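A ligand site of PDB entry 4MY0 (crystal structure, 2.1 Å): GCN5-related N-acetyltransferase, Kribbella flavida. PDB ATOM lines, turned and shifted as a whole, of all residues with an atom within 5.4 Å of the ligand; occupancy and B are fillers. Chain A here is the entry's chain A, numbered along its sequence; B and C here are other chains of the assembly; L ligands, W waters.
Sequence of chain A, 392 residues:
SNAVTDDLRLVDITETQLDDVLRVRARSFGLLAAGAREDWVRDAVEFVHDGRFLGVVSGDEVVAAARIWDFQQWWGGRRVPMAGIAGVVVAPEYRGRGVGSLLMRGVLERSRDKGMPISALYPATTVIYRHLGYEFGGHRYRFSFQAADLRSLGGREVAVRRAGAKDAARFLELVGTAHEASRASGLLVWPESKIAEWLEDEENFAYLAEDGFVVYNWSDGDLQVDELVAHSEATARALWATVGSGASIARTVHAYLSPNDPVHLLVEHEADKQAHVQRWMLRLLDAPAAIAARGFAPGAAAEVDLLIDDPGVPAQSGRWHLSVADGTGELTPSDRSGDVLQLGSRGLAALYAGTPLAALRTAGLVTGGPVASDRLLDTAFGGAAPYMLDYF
The backbone NH of Ser 101 lies within hydrogen-bond range of an oxygen (O8) of the ligand, 3.0 Å away.
OG of Ser 101 lies within hydrogen-bond range of O8 of the ligand (2.4 Å).
OG of Ser 248 of chain B lies within hydrogen-bond range of O16 of the ligand (2.5 Å).
An oxygen (O9) of the ligand is in hydrogen-bond range of the backbone NH (N) of Gly 98, at 2.7 Å.
The backbone carbonyl oxygen (O) of Val 88 lies within hydrogen-bond range of a nitrogen (N7) of the ligand (2.7 Å).
The backbone NH (N) of Gly 100 is in hydrogen-bond range of an oxygen (O11) of the ligand.
The side-chain hydroxyl (OH) of Tyr 129 lies close to a sulfur (S1) of the ligand, 2.9 Å away.
The backbone NH (N) of Gly 96 lies within hydrogen-bond range of an oxygen (O12) of the ligand.
A ring nitrogen (NE2) of His 131 is in hydrogen-bond range of an oxygen (O4) of the ligand.
NH1 of Arg 151 of chain B is in hydrogen-bond range of O1 of the ligand (2.9 Å).
An oxygen (O15) of the ligand sits at hydrogen-bond distance from the backbone NH (N) of Val 90, 3.0 Å away.
The backbone NH (N) of Arg 97 sits at hydrogen-bond distance from an oxygen (O9) of the ligand.
NE of Arg 95 sits at hydrogen-bond distance from O15 of the ligand (3.3 Å).
The backbone NH (N) of Ala 124 lies close to a sulfur (S1) of the ligand (3.4 Å).
CB of Ser 28 touches C18 of the ligand, 3.8 Å away.
CE2 of Phe 29 touches C20 of the ligand, 3.6 Å away.
Val 89 touches the ligand.
N of Val 99 touches O11 of the ligand (3.7 Å).
Thr 125 touches the ligand (CG2 to C14, 3.7 Å).
Val 127 touches the ligand.
Ile 128 touches the ligand (N to O6, 3.6 Å).
Ile 249 of chain B touches the ligand (CG1 to O16, 3.6 Å).
OE1 of Glu 268 of chain C touches C1 of the ligand, 3.2 Å away.
Hydrophobic or aromatic side chains that line the ligand: Phe 29, Val 88, Val 90, Ala 124, Val 127, Ile 128, Tyr 129, His 131 and Ile 249 of chain B.
22 residues have an atom within 4 Å of the ligand: Ser 28, Phe 29, Val 88, Val 89, Val 90, Arg 95, Gly 96, Arg 97, Gly 98, Val 99, Gly 100, Ser 101, Ala 124, Thr 125, Val 127, Ile 128, Tyr 129, His 131, Arg 151 of chain B, Ser 248 of chain B, Ile 249 of chain B and Glu 268 of chain C.
The nearest printed residue that does not touch the ligand is Tyr 122 (4.03 Å).
O of Val 90 lies within hydrogen-bond range of NE of Arg 95 (2.8 Å).
NH2 of Arg 95 is in hydrogen-bond range of OG of Ser 28 (3.0 Å).
The guanidinium group (NH1) of Arg 95 lies within hydrogen-bond range of the side-chain hydroxyl (OG) of Ser 245 of chain B (2.9 Å).
Water W4 lies within hydrogen-bond range of an oxygen (O9) of the ligand and the backbone carbonyl oxygen (O) of Gly 96.
Water W9 lies within hydrogen-bond range of OG of Ser 248 of chain B (2.6 Å), O of Ser 245 of chain B (2.7 Å) and N3 of the ligand (2.8 Å).
Water W3 lies within hydrogen-bond range of O1 of the ligand and NH1 of Arg 151 of chain B.
Water W1 lies within hydrogen-bond range of N4 of the ligand (3.0 Å), NE of Arg 151 of chain B (3.0 Å) and O of Ser 245 of chain B (3.3 Å).
Water W11 lies within hydrogen-bond range of the side-chain hydroxyl of Thr 125, the side-chain carboxylate of Glu 268 of chain C and a nitrogen (N1) of the ligand.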
ATOM      1  N   SER A  28      14.380 -15.404 -17.834  1.00  0.00           N
ATOM      2  CA  SER A  28      12.948 -15.666 -17.694  1.00  0.00           C
ATOM      3  C   SER A  28      12.127 -14.420 -17.359  1.00  0.00           C
ATOM      4  O   SER A  28      11.139 -14.136 -18.056  1.00  0.00           O
ATOM      5  CB  SER A  28      12.703 -16.753 -16.653  1.00  0.00           C
ATOM      6  OG  SER A  28      13.286 -17.979 -17.070  1.00  0.00           O
ATOM      7  N   PHE A  29      12.519 -13.696 -16.319  1.00  0.00           N
ATOM      8  CA  PHE A  29      11.764 -12.514 -15.876  1.00  0.00           C
ATOM      9  C   PHE A  29      12.441 -11.208 -16.236  1.00  0.00           C
ATOM     10  O   PHE A  29      11.783 -10.161 -16.307  1.00  0.00           O
ATOM     11  CB  PHE A  29      11.564 -12.522 -14.349  1.00  0.00           C
ATOM     12  CG  PHE A  29      10.771 -13.689 -13.836  1.00  0.00           C
ATOM     13  CD1 PHE A  29      11.088 -14.272 -12.602  1.00  0.00           C
ATOM     14  CD2 PHE A  29       9.712 -14.207 -14.568  1.00  0.00           C
ATOM     15  CE1 PHE A  29      10.365 -15.354 -12.119  1.00  0.00           C
ATOM     16  CE2 PHE A  29       8.977 -15.286 -14.094  1.00  0.00           C
ATOM     17  CZ  PHE A  29       9.307 -15.865 -12.864  1.00  0.00           C
ATOM     18  N   VAL A  88       8.761 -19.461 -10.720  1.00  0.00           N
ATOM     19  CA  VAL A  88       8.846 -20.645 -11.566  1.00  0.00           C
ATOM     20  C   VAL A  88       9.527 -20.270 -12.868  1.00  0.00           C
ATOM     21  O   VAL A  88       8.987 -19.483 -13.655  1.00  0.00           O
ATOM     22  CB  VAL A  88       7.443 -21.205 -11.861  1.00  0.00           C
ATOM     23  CG1 VAL A  88       7.540 -22.423 -12.804  1.00  0.00           C
ATOM     24  CG2 VAL A  88       6.739 -21.581 -10.555  1.00  0.00           C
ATOM     25  N   VAL A  89      10.722 -20.809 -13.090  1.00  0.00           N
ATOM     26  CA  VAL A  89      11.511 -20.431 -14.265  1.00  0.00           C
ATOM     27  C   VAL A  89      12.128 -21.649 -14.916  1.00  0.00           C
ATOM     28  O   VAL A  89      12.545 -22.580 -14.222  1.00  0.00           O
ATOM     29  CB  VAL A  89      12.640 -19.436 -13.879  1.00  0.00           C
ATOM     30  CG1 VAL A  89      12.063 -18.095 -13.479  1.00  0.00           C
ATOM     31  CG2 VAL A  89      13.492 -20.014 -12.732  1.00  0.00           C
ATOM     32  N   VAL A  90      12.175 -21.666 -16.248  1.00  0.00           N
ATOM     33  CA  VAL A  90      12.836 -22.720 -17.006  1.00  0.00           C
ATOM     34  C   VAL A  90      13.765 -22.069 -18.046  1.00  0.00           C
ATOM     35  O   VAL A  90      13.356 -21.099 -18.709  1.00  0.00           O
ATOM     36  CB  VAL A  90      11.818 -23.613 -17.764  1.00  0.00           C
ATOM     37  CG1 VAL A  90      12.552 -24.607 -18.672  1.00  0.00           C
ATOM     38  CG2 VAL A  90      10.910 -24.359 -16.788  1.00  0.00           C
ATOM     39  N   ALA A  91      14.987 -22.582 -18.175  1.00  0.00           N
ATOM     40  CA  ALA A  91      15.941 -22.076 -19.176  1.00  0.00           C
ATOM     41  C   ALA A  91      15.349 -22.139 -20.594  1.00  0.00           C
ATOM     42  O   ALA A  91      14.736 -23.132 -20.957  1.00  0.00           O
ATOM     43  CB  ALA A  91      17.244 -22.901 -19.102  1.00  0.00           C
ATOM     44  N   TYR A  94      15.425 -25.106 -22.736  1.00  0.00           N
ATOM     45  CA  TYR A  94      14.793 -26.292 -22.130  1.00  0.00           C
ATOM     46  C   TYR A  94      13.279 -26.170 -21.991  1.00  0.00           C
ATOM     47  O   TYR A  94      12.638 -27.052 -21.400  1.00  0.00           O
ATOM     48  CB  TYR A  94      15.440 -26.618 -20.768  1.00  0.00           C
ATOM     49  CG  TYR A  94      16.817 -27.253 -20.862  1.00  0.00           C
ATOM     50  CD1 TYR A  94      16.970 -28.626 -20.794  1.00  0.00           C
ATOM     51  CD2 TYR A  94      17.959 -26.482 -21.030  1.00  0.00           C
ATOM     52  CE1 TYR A  94      18.227 -29.212 -20.891  1.00  0.00           C
ATOM     53  CE2 TYR A  94      19.215 -27.046 -21.132  1.00  0.00           C
ATOM     54  CZ  TYR A  94      19.349 -28.411 -21.063  1.00  0.00           C
ATOM     55  OH  TYR A  94      20.605 -28.974 -21.164  1.00  0.00           O
ATOM     56  N   ARG A  95      12.696 -25.113 -22.532  1.00  0.00           N
ATOM     57  CA  ARG A  95      11.241 -24.901 -22.423  1.00  0.00           C
ATOM     58  C   ARG A  95      10.518 -25.759 -23.443  1.00  0.00           C
ATOM     59  O   ARG A  95      11.129 -26.234 -24.407  1.00  0.00           O
ATOM     60  CB  ARG A  95      10.884 -23.428 -22.637  1.00  0.00           C
ATOM     61  CG  ARG A  95      11.292 -22.532 -21.483  1.00  0.00           C
ATOM     62  CD  ARG A  95      11.162 -21.047 -21.829  1.00  0.00           C
ATOM     63  NE  ARG A  95      11.800 -20.208 -20.802  1.00  0.00           N
ATOM     64  CZ  ARG A  95      12.233 -18.979 -21.013  1.00  0.00           C
ATOM     65  NH1 ARG A  95      12.117 -18.414 -22.212  1.00  0.00           N
ATOM     66  NH2 ARG A  95      12.803 -18.290 -20.024  1.00  0.00           N
ATOM     67  N   GLY A  96       9.227 -26.008 -23.245  1.00  0.00           N
ATOM     68  CA  GLY A  96       8.448 -26.695 -24.263  1.00  0.00           C
ATOM     69  C   GLY A  96       8.784 -28.172 -24.398  1.00  0.00           C
ATOM     70  O   GLY A  96       8.462 -28.793 -25.410  1.00  0.00           O
ATOM     71  N   ARG A  97       9.429 -28.729 -23.367  1.00  0.00           N
ATOM     72  CA  ARG A  97       9.835 -30.132 -23.415  1.00  0.00           C
ATOM     73  C   ARG A  97       9.412 -30.884 -22.141  1.00  0.00           C
ATOM     74  O   ARG A  97       9.916 -31.962 -21.863  1.00  0.00           O
ATOM     75  CB  ARG A  97      11.362 -30.251 -23.567  1.00  0.00           C
ATOM     76  CG  ARG A  97      11.942 -29.661 -24.860  1.00  0.00           C
ATOM     77  CD  ARG A  97      13.481 -29.676 -24.830  1.00  0.00           C
ATOM     78  NE  ARG A  97      13.989 -30.763 -24.001  1.00  0.00           N
ATOM     79  CZ  ARG A  97      15.275 -31.050 -23.807  1.00  0.00           C
ATOM     80  NH1 ARG A  97      16.215 -30.332 -24.408  1.00  0.00           N
ATOM     81  NH2 ARG A  97      15.638 -32.066 -23.022  1.00  0.00           N
ATOM     82  N   GLY A  98       8.498 -30.303 -21.371  1.00  0.00           N
ATOM     83  CA  GLY A  98       8.005 -30.957 -20.171  1.00  0.00           C
ATOM     84  C   GLY A  98       8.812 -30.736 -18.896  1.00  0.00           C
ATOM     85  O   GLY A  98       8.495 -31.293 -17.838  1.00  0.00           O
ATOM     86  N   VAL A  99       9.850 -29.910 -18.987  1.00  0.00           N
ATOM     87  CA  VAL A  99      10.703 -29.642 -17.834  1.00  0.00           C
ATOM     88  C   VAL A  99       9.937 -28.894 -16.741  1.00  0.00           C
ATOM     89  O   VAL A  99      10.024 -29.248 -15.554  1.00  0.00           O
ATOM     90  CB  VAL A  99      11.976 -28.891 -18.225  1.00  0.00           C
ATOM     91  CG1 VAL A  99      12.747 -28.425 -16.979  1.00  0.00           C
ATOM     92  CG2 VAL A  99      12.856 -29.782 -19.106  1.00  0.00           C
ATOM     93  N   GLY A 100       9.161 -27.895 -17.145  1.00  0.00           N
ATOM     94  CA  GLY A 100       8.380 -27.110 -16.214  1.00  0.00           C
ATOM     95  C   GLY A 100       7.394 -27.978 -15.457  1.00  0.00           C
ATOM     96  O   GLY A 100       7.188 -27.785 -14.255  1.00  0.00           O
ATOM     97  N   SER A 101       6.780 -28.928 -16.173  1.00  0.00           N
ATOM     98  CA  SER A 101       5.790 -29.831 -15.584  1.00  0.00           C
ATOM     99  C   SER A 101       6.431 -30.815 -14.592  1.00  0.00           C
ATOM    100  O   SER A 101       5.871 -31.084 -13.520  1.00  0.00           O
ATOM    101  CB  SER A 101       5.052 -30.587 -16.698  1.00  0.00           C
ATOM    102  OG  SER A 101       4.383 -29.686 -17.553  1.00  0.00           O
ATOM    103  N   LEU A 102       7.593 -31.334 -14.948  1.00  0.00           N
ATOM    104  CA  LEU A 102       8.368 -32.201 -14.055  1.00  0.00           C
ATOM    105  C   LEU A 102       8.720 -31.447 -12.777  1.00  0.00           C
ATOM    106  O   LEU A 102       8.625 -31.981 -11.666  1.00  0.00           O
ATOM    107  CB  LEU A 102       9.638 -32.653 -14.755  1.00  0.00           C
ATOM    108  CG  LEU A 102      10.659 -33.491 -13.980  1.00  0.00           C
ATOM    109  CD1 LEU A 102      10.099 -34.856 -13.614  1.00  0.00           C
ATOM    110  CD2 LEU A 102      11.930 -33.630 -14.802  1.00  0.00           C
ATOM    111  N   TYR A 122       0.232 -17.004  -8.675  1.00  0.00           N
ATOM    112  CA  TYR A 122      -0.184 -16.075  -9.722  1.00  0.00           C
ATOM    113  C   TYR A 122       0.503 -16.508 -11.008  1.00  0.00           C
ATOM    114  O   TYR A 122       1.729 -16.444 -11.123  1.00  0.00           O
ATOM    115  CB  TYR A 122       0.297 -14.656  -9.403  1.00  0.00           C
ATOM    116  CG  TYR A 122      -0.506 -13.886  -8.361  1.00  0.00           C
ATOM    117  CD1 TYR A 122      -1.543 -13.036  -8.732  1.00  0.00           C
ATOM    118  CD2 TYR A 122      -0.189 -13.987  -7.019  1.00  0.00           C
ATOM    119  CE1 TYR A 122      -2.252 -12.312  -7.788  1.00  0.00           C
ATOM    120  CE2 TYR A 122      -0.895 -13.283  -6.061  1.00  0.00           C
ATOM    121  CZ  TYR A 122      -1.925 -12.441  -6.451  1.00  0.00           C
ATOM    122  OH  TYR A 122      -2.627 -11.723  -5.517  1.00  0.00           O
ATOM    123  N   PRO A 123      -0.286 -16.976 -11.981  1.00  0.00           N
ATOM    124  CA  PRO A 123       0.352 -17.610 -13.142  1.00  0.00           C
ATOM    125  C   PRO A 123       0.656 -16.603 -14.258  1.00  0.00           C
ATOM    126  O   PRO A 123      -0.179 -15.731 -14.530  1.00  0.00           O
ATOM    127  CB  PRO A 123      -0.724 -18.595 -13.611  1.00  0.00           C
ATOM    128  CG  PRO A 123      -2.056 -17.832 -13.324  1.00  0.00           C
ATOM    129  CD  PRO A 123      -1.762 -17.118 -11.996  1.00  0.00           C
ATOM    130  N   ALA A 124       1.815 -16.721 -14.901  1.00  0.00           N
ATOM    131  CA  ALA A 124       2.096 -15.904 -16.084  1.00  0.00           C
ATOM    132  C   ALA A 124       1.412 -16.500 -17.304  1.00  0.00           C
ATOM    133  O   ALA A 124       1.042 -15.780 -18.228  1.00  0.00           O
ATOM    134  CB  ALA A 124       3.601 -15.786 -16.338  1.00  0.00           C
ATOM    135  N   THR A 125       1.294 -17.829 -17.328  1.00  0.00           N
ATOM    136  CA  THR A 125       0.543 -18.525 -18.370  1.00  0.00           C
ATOM    137  C   THR A 125      -0.327 -19.545 -17.660  1.00  0.00           C
ATOM    138  O   THR A 125       0.129 -20.196 -16.723  1.00  0.00           O
ATOM    139  CB  THR A 125       1.487 -19.227 -19.397  1.00  0.00           C
ATOM    140  OG1 THR A 125       0.716 -20.092 -20.242  1.00  0.00           O
ATOM    141  CG2 THR A 125       2.560 -20.038 -18.688  1.00  0.00           C
ATOM    142  N   VAL A 127      -1.801 -22.262 -18.971  1.00  0.00           N
ATOM    143  CA  VAL A 127      -1.874 -23.615 -19.545  1.00  0.00           C
ATOM    144  C   VAL A 127      -1.195 -24.671 -18.667  1.00  0.00           C
ATOM    145  O   VAL A 127      -1.834 -25.672 -18.288  1.00  0.00           O
ATOM    146  CB  VAL A 127      -1.321 -23.687 -20.986  1.00  0.00           C
ATOM    147  CG1 VAL A 127      -1.462 -25.121 -21.552  1.00  0.00           C
ATOM    148  CG2 VAL A 127      -2.051 -22.694 -21.883  1.00  0.00           C
ATOM    149  N   ILE A 128       0.070 -24.455 -18.324  1.00  0.00           N
ATOM    150  CA  ILE A 128       0.810 -25.457 -17.561  1.00  0.00           C
ATOM    151  C   ILE A 128       0.118 -25.713 -16.211  1.00  0.00           C
ATOM    152  O   ILE A 128       0.011 -26.855 -15.770  1.00  0.00           O
ATOM    153  CB  ILE A 128       2.299 -25.063 -17.356  1.00  0.00           C
ATOM    154  CG1 ILE A 128       3.054 -26.197 -16.638  1.00  0.00           C
ATOM    155  CG2 ILE A 128       2.442 -23.726 -16.581  1.00  0.00           C
ATOM    156  CD1 ILE A 128       4.552 -25.972 -16.500  1.00  0.00           C
ATOM    157  N   TYR A 129      -0.390 -24.668 -15.569  1.00  0.00           N
ATOM    158  CA  TYR A 129      -0.975 -24.852 -14.242  1.00  0.00           C
ATOM    159  C   TYR A 129      -2.355 -25.541 -14.294  1.00  0.00           C
ATOM    160  O   TYR A 129      -2.676 -26.354 -13.427  1.00  0.00           O
ATOM    161  CB  TYR A 129      -0.995 -23.541 -13.446  1.00  0.00           C
ATOM    162  CG  TYR A 129       0.381 -22.920 -13.326  1.00  0.00           C
ATOM    163  CD1 TYR A 129       1.361 -23.508 -12.528  1.00  0.00           C
ATOM    164  CD2 TYR A 129       0.727 -21.770 -14.045  1.00  0.00           C
ATOM    165  CE1 TYR A 129       2.629 -22.981 -12.422  1.00  0.00           C
ATOM    166  CE2 TYR A 129       1.999 -21.210 -13.937  1.00  0.00           C
ATOM    167  CZ  TYR A 129       2.943 -21.832 -13.115  1.00  0.00           C
ATOM    168  OH  TYR A 129       4.213 -21.302 -13.000  1.00  0.00           O
ATOM    169  N   HIS A 131      -3.209 -27.769 -16.570  1.00  0.00           N
ATOM    170  CA  HIS A 131      -2.847 -29.176 -16.776  1.00  0.00           C
ATOM    171  C   HIS A 131      -2.466 -29.826 -15.445  1.00  0.00           C
ATOM    172  O   HIS A 131      -2.684 -31.014 -15.246  1.00  0.00           O
ATOM    173  CB  HIS A 131      -1.658 -29.333 -17.738  1.00  0.00           C
ATOM    174  CG  HIS A 131      -2.015 -29.158 -19.194  1.00  0.00           C
ATOM    175  ND1 HIS A 131      -3.222 -29.541 -19.716  1.00  0.00           N
ATOM    176  CD2 HIS A 131      -1.303 -28.650 -20.230  1.00  0.00           C
ATOM    177  CE1 HIS A 131      -3.246 -29.278 -21.006  1.00  0.00           C
ATOM    178  NE2 HIS A 131      -2.093 -28.730 -21.342  1.00  0.00           N
ATOM    179  N   ARG B 151       6.992 -18.462 -30.769  1.00  0.00           N
ATOM    180  CA  ARG B 151       7.033 -19.645 -29.907  1.00  0.00           C
ATOM    181  C   ARG B 151       6.552 -20.916 -30.602  1.00  0.00           C
ATOM    182  O   ARG B 151       7.086 -21.994 -30.360  1.00  0.00           O
ATOM    183  CB  ARG B 151       6.209 -19.425 -28.624  1.00  0.00           C
ATOM    184  CG  ARG B 151       6.295 -20.644 -27.667  1.00  0.00           C
ATOM    185  CD  ARG B 151       5.443 -20.479 -26.418  1.00  0.00           C
ATOM    186  NE  ARG B 151       5.247 -21.774 -25.784  1.00  0.00           N
ATOM    187  CZ  ARG B 151       4.201 -22.548 -26.025  1.00  0.00           C
ATOM    188  NH1 ARG B 151       4.100 -23.723 -25.421  1.00  0.00           N
ATOM    189  NH2 ARG B 151       3.249 -22.140 -26.859  1.00  0.00           N
ATOM    190  N   SER B 245       9.899 -18.503 -26.769  1.00  0.00           N
ATOM    191  CA  SER B 245       9.500 -19.354 -25.642  1.00  0.00           C
ATOM    192  C   SER B 245       9.223 -18.509 -24.389  1.00  0.00           C
ATOM    193  O   SER B 245       8.590 -18.976 -23.447  1.00  0.00           O
ATOM    194  CB  SER B 245      10.558 -20.416 -25.351  1.00  0.00           C
ATOM    195  OG  SER B 245      11.687 -19.829 -24.708  1.00  0.00           O
ATOM    196  N   GLY B 246       9.689 -17.256 -24.393  1.00  0.00           N
ATOM    197  CA  GLY B 246       9.493 -16.388 -23.251  1.00  0.00           C
ATOM    198  C   GLY B 246       8.201 -15.584 -23.343  1.00  0.00           C
ATOM    199  O   GLY B 246       8.003 -14.618 -22.597  1.00  0.00           O
ATOM    200  N   ALA B 247       7.323 -15.988 -24.265  1.00  0.00           N
ATOM    201  CA  ALA B 247       6.064 -15.284 -24.537  1.00  0.00           C
ATOM    202  C   ALA B 247       5.158 -15.091 -23.307  1.00  0.00           C
ATOM    203  O   ALA B 247       4.307 -14.219 -23.297  1.00  0.00           O
ATOM    204  CB  ALA B 247       5.284 -15.987 -25.645  1.00  0.00           C
ATOM    205  N   SER B 248       5.328 -15.932 -22.283  1.00  0.00           N
ATOM    206  CA  SER B 248       4.471 -15.819 -21.105  1.00  0.00           C
ATOM    207  C   SER B 248       4.721 -14.507 -20.372  1.00  0.00           C
ATOM    208  O   SER B 248       3.868 -14.031 -19.640  1.00  0.00           O
ATOM    209  CB  SER B 248       4.662 -16.997 -20.163  1.00  0.00           C
ATOM    210  OG  SER B 248       6.036 -17.240 -19.920  1.00  0.00           O
ATOM    211  N   ILE B 249       5.899 -13.917 -20.608  1.00  0.00           N
ATOM    212  CA  ILE B 249       6.323 -12.670 -19.961  1.00  0.00           C
ATOM    213  C   ILE B 249       6.499 -11.546 -20.979  1.00  0.00           C
ATOM    214  O   ILE B 249       6.079 -10.420 -20.742  1.00  0.00           O
ATOM    215  CB  ILE B 249       7.697 -12.848 -19.266  1.00  0.00           C
ATOM    216  CG1 ILE B 249       7.631 -13.953 -18.218  1.00  0.00           C
ATOM    217  CG2 ILE B 249       8.125 -11.520 -18.607  1.00  0.00           C
ATOM    218  CD1 ILE B 249       6.711 -13.609 -17.072  1.00  0.00           C
ATOM    219  N   GLU C 268      -7.695 -18.989 -22.649  1.00  0.00           N
ATOM    220  CA  GLU C 268      -6.308 -19.270 -22.286  1.00  0.00           C
ATOM    221  C   GLU C 268      -5.652 -18.073 -21.592  1.00  0.00           C
ATOM    222  O   GLU C 268      -4.964 -18.212 -20.569  1.00  0.00           O
ATOM    223  CB  GLU C 268      -5.495 -19.648 -23.511  1.00  0.00           C
ATOM    224  CG  GLU C 268      -3.999 -19.725 -23.180  1.00  0.00           C
ATOM    225  CD  GLU C 268      -3.124 -20.141 -24.365  1.00  0.00           C
ATOM    226  OE1 GLU C 268      -1.894 -19.892 -24.304  1.00  0.00           O
ATOM    227  OE2 GLU C 268      -3.667 -20.722 -25.331  1.00  0.00           O
HETATM  228  N1  LIG L   1       1.999 -20.138 -23.836  1.00  0.00           N
HETATM  229  C1  LIG L   1       1.094 -21.125 -23.989  1.00  0.00           C
HETATM  230  N2  LIG L   1       1.289 -22.379 -23.529  1.00  0.00           N
HETATM  231  C2  LIG L   1       2.430 -22.731 -22.882  1.00  0.00           C
HETATM  232  C3  LIG L   1       3.465 -21.704 -22.676  1.00  0.00           C
HETATM  233  C4  LIG L   1       3.182 -20.344 -23.208  1.00  0.00           C
HETATM  234  N3  LIG L   1       4.094 -19.338 -23.061  1.00  0.00           N
HETATM  235  N4  LIG L   1       4.477 -22.301 -22.016  1.00  0.00           N
HETATM  236  C5  LIG L   1       4.121 -23.605 -21.800  1.00  0.00           C
HETATM  237  N5  LIG L   1       2.907 -23.853 -22.331  1.00  0.00           N
HETATM  238  C6  LIG L   1       2.197 -25.145 -22.279  1.00  0.00           C
HETATM  239  C7  LIG L   1       2.903 -26.187 -23.120  1.00  0.00           C
HETATM  240  O1  LIG L   1       2.580 -26.065 -24.518  1.00  0.00           O
HETATM  241  C8  LIG L   1       2.372 -27.448 -22.471  1.00  0.00           C
HETATM  242  O2  LIG L   1       1.012 -27.601 -22.855  1.00  0.00           O
HETATM  243  P1  LIG L   1       0.534 -28.633 -23.998  1.00  0.00           P
HETATM  244  O3  LIG L   1       0.984 -29.987 -23.473  1.00  0.00           O
HETATM  245  O4  LIG L   1      -0.968 -28.433 -24.035  1.00  0.00           O
HETATM  246  O5  LIG L   1       1.278 -28.175 -25.236  1.00  0.00           O
HETATM  247  C9  LIG L   1       2.285 -27.122 -20.986  1.00  0.00           C
HETATM  248  O6  LIG L   1       2.257 -25.680 -20.944  1.00  0.00           O
HETATM  249  C10 LIG L   1       3.449 -27.692 -20.169  1.00  0.00           C
HETATM  250  O7  LIG L   1       4.653 -27.496 -20.901  1.00  0.00           O
HETATM  251  P2  LIG L   1       6.115 -27.692 -20.258  1.00  0.00           P
HETATM  252  O8  LIG L   1       5.969 -28.579 -19.039  1.00  0.00           O
HETATM  253  O9  LIG L   1       7.047 -28.036 -21.385  1.00  0.00           O
HETATM  254  O10 LIG L   1       6.406 -26.183 -19.753  1.00  0.00           O
HETATM  255  P3  LIG L   1       7.796 -25.384 -19.810  1.00  0.00           P
HETATM  256  O11 LIG L   1       8.933 -26.326 -19.455  1.00  0.00           O
HETATM  257  O12 LIG L   1       7.912 -24.610 -21.072  1.00  0.00           O
HETATM  258  O13 LIG L   1       7.591 -24.377 -18.553  1.00  0.00           O
HETATM  259  C11 LIG L   1       7.209 -22.045 -18.179  1.00  0.00           C
HETATM  260  C12 LIG L   1       6.579 -23.369 -18.580  1.00  0.00           C
HETATM  261  C13 LIG L   1       7.653 -22.076 -16.718  1.00  0.00           C
HETATM  262  C14 LIG L   1       6.151 -20.966 -18.412  1.00  0.00           C
HETATM  263  C15 LIG L   1       8.434 -21.787 -19.053  1.00  0.00           C
HETATM  264  O14 LIG L   1       8.029 -21.827 -20.433  1.00  0.00           O
HETATM  265  C16 LIG L   1       9.131 -20.473 -18.745  1.00  0.00           C
HETATM  266  O15 LIG L   1      10.126 -20.470 -18.020  1.00  0.00           O
HETATM  267  N6  LIG L   1       8.652 -19.356 -19.274  1.00  0.00           N
HETATM  268  C17 LIG L   1       9.144 -18.008 -18.992  1.00  0.00           C
HETATM  269  C18 LIG L   1       9.126 -17.598 -17.506  1.00  0.00           C
HETATM  270  C19 LIG L   1       7.739 -17.741 -16.933  1.00  0.00           C
HETATM  271  O16 LIG L   1       6.756 -17.358 -17.549  1.00  0.00           O
HETATM  272  N7  LIG L   1       7.634 -18.285 -15.715  1.00  0.00           N
HETATM  273  C20 LIG L   1       6.592 -17.894 -14.778  1.00  0.00           C
HETATM  274  C21 LIG L   1       5.422 -18.853 -14.792  1.00  0.00           C
HETATM  275  S1  LIG L   1       4.321 -18.446 -13.465  1.00  0.00           S
HETATM  276  O   HOH W   1       7.132 -21.885 -23.390  1.00  0.00           O
HETATM  277  O   HOH W   2      -0.308 -24.121 -25.145  1.00  0.00           O
HETATM  278  O   HOH W   3       1.406 -24.930 -26.995  1.00  0.00           O
HETATM  279  O   HOH W   4       5.789 -29.107 -23.600  1.00  0.00           O
HETATM  280  O   HOH W   5       1.639 -17.101 -22.598  1.00  0.00           O
HETATM  281  O   HOH W   6      -1.979 -26.464 -24.964  1.00  0.00           O
HETATM  282  O   HOH W   7       1.516 -30.851 -20.924  1.00  0.00           O
HETATM  283  O   HOH W   8      10.198 -27.937 -21.044  1.00  0.00           O
HETATM  284  O   HOH W   9       6.555 -19.073 -21.735  1.00  0.00           O
HETATM  285  O   HOH W  10       1.801 -18.518 -26.007  1.00  0.00           O
HETATM  286  O   HOH W  11      -0.574 -18.746 -22.168  1.00  0.00           O
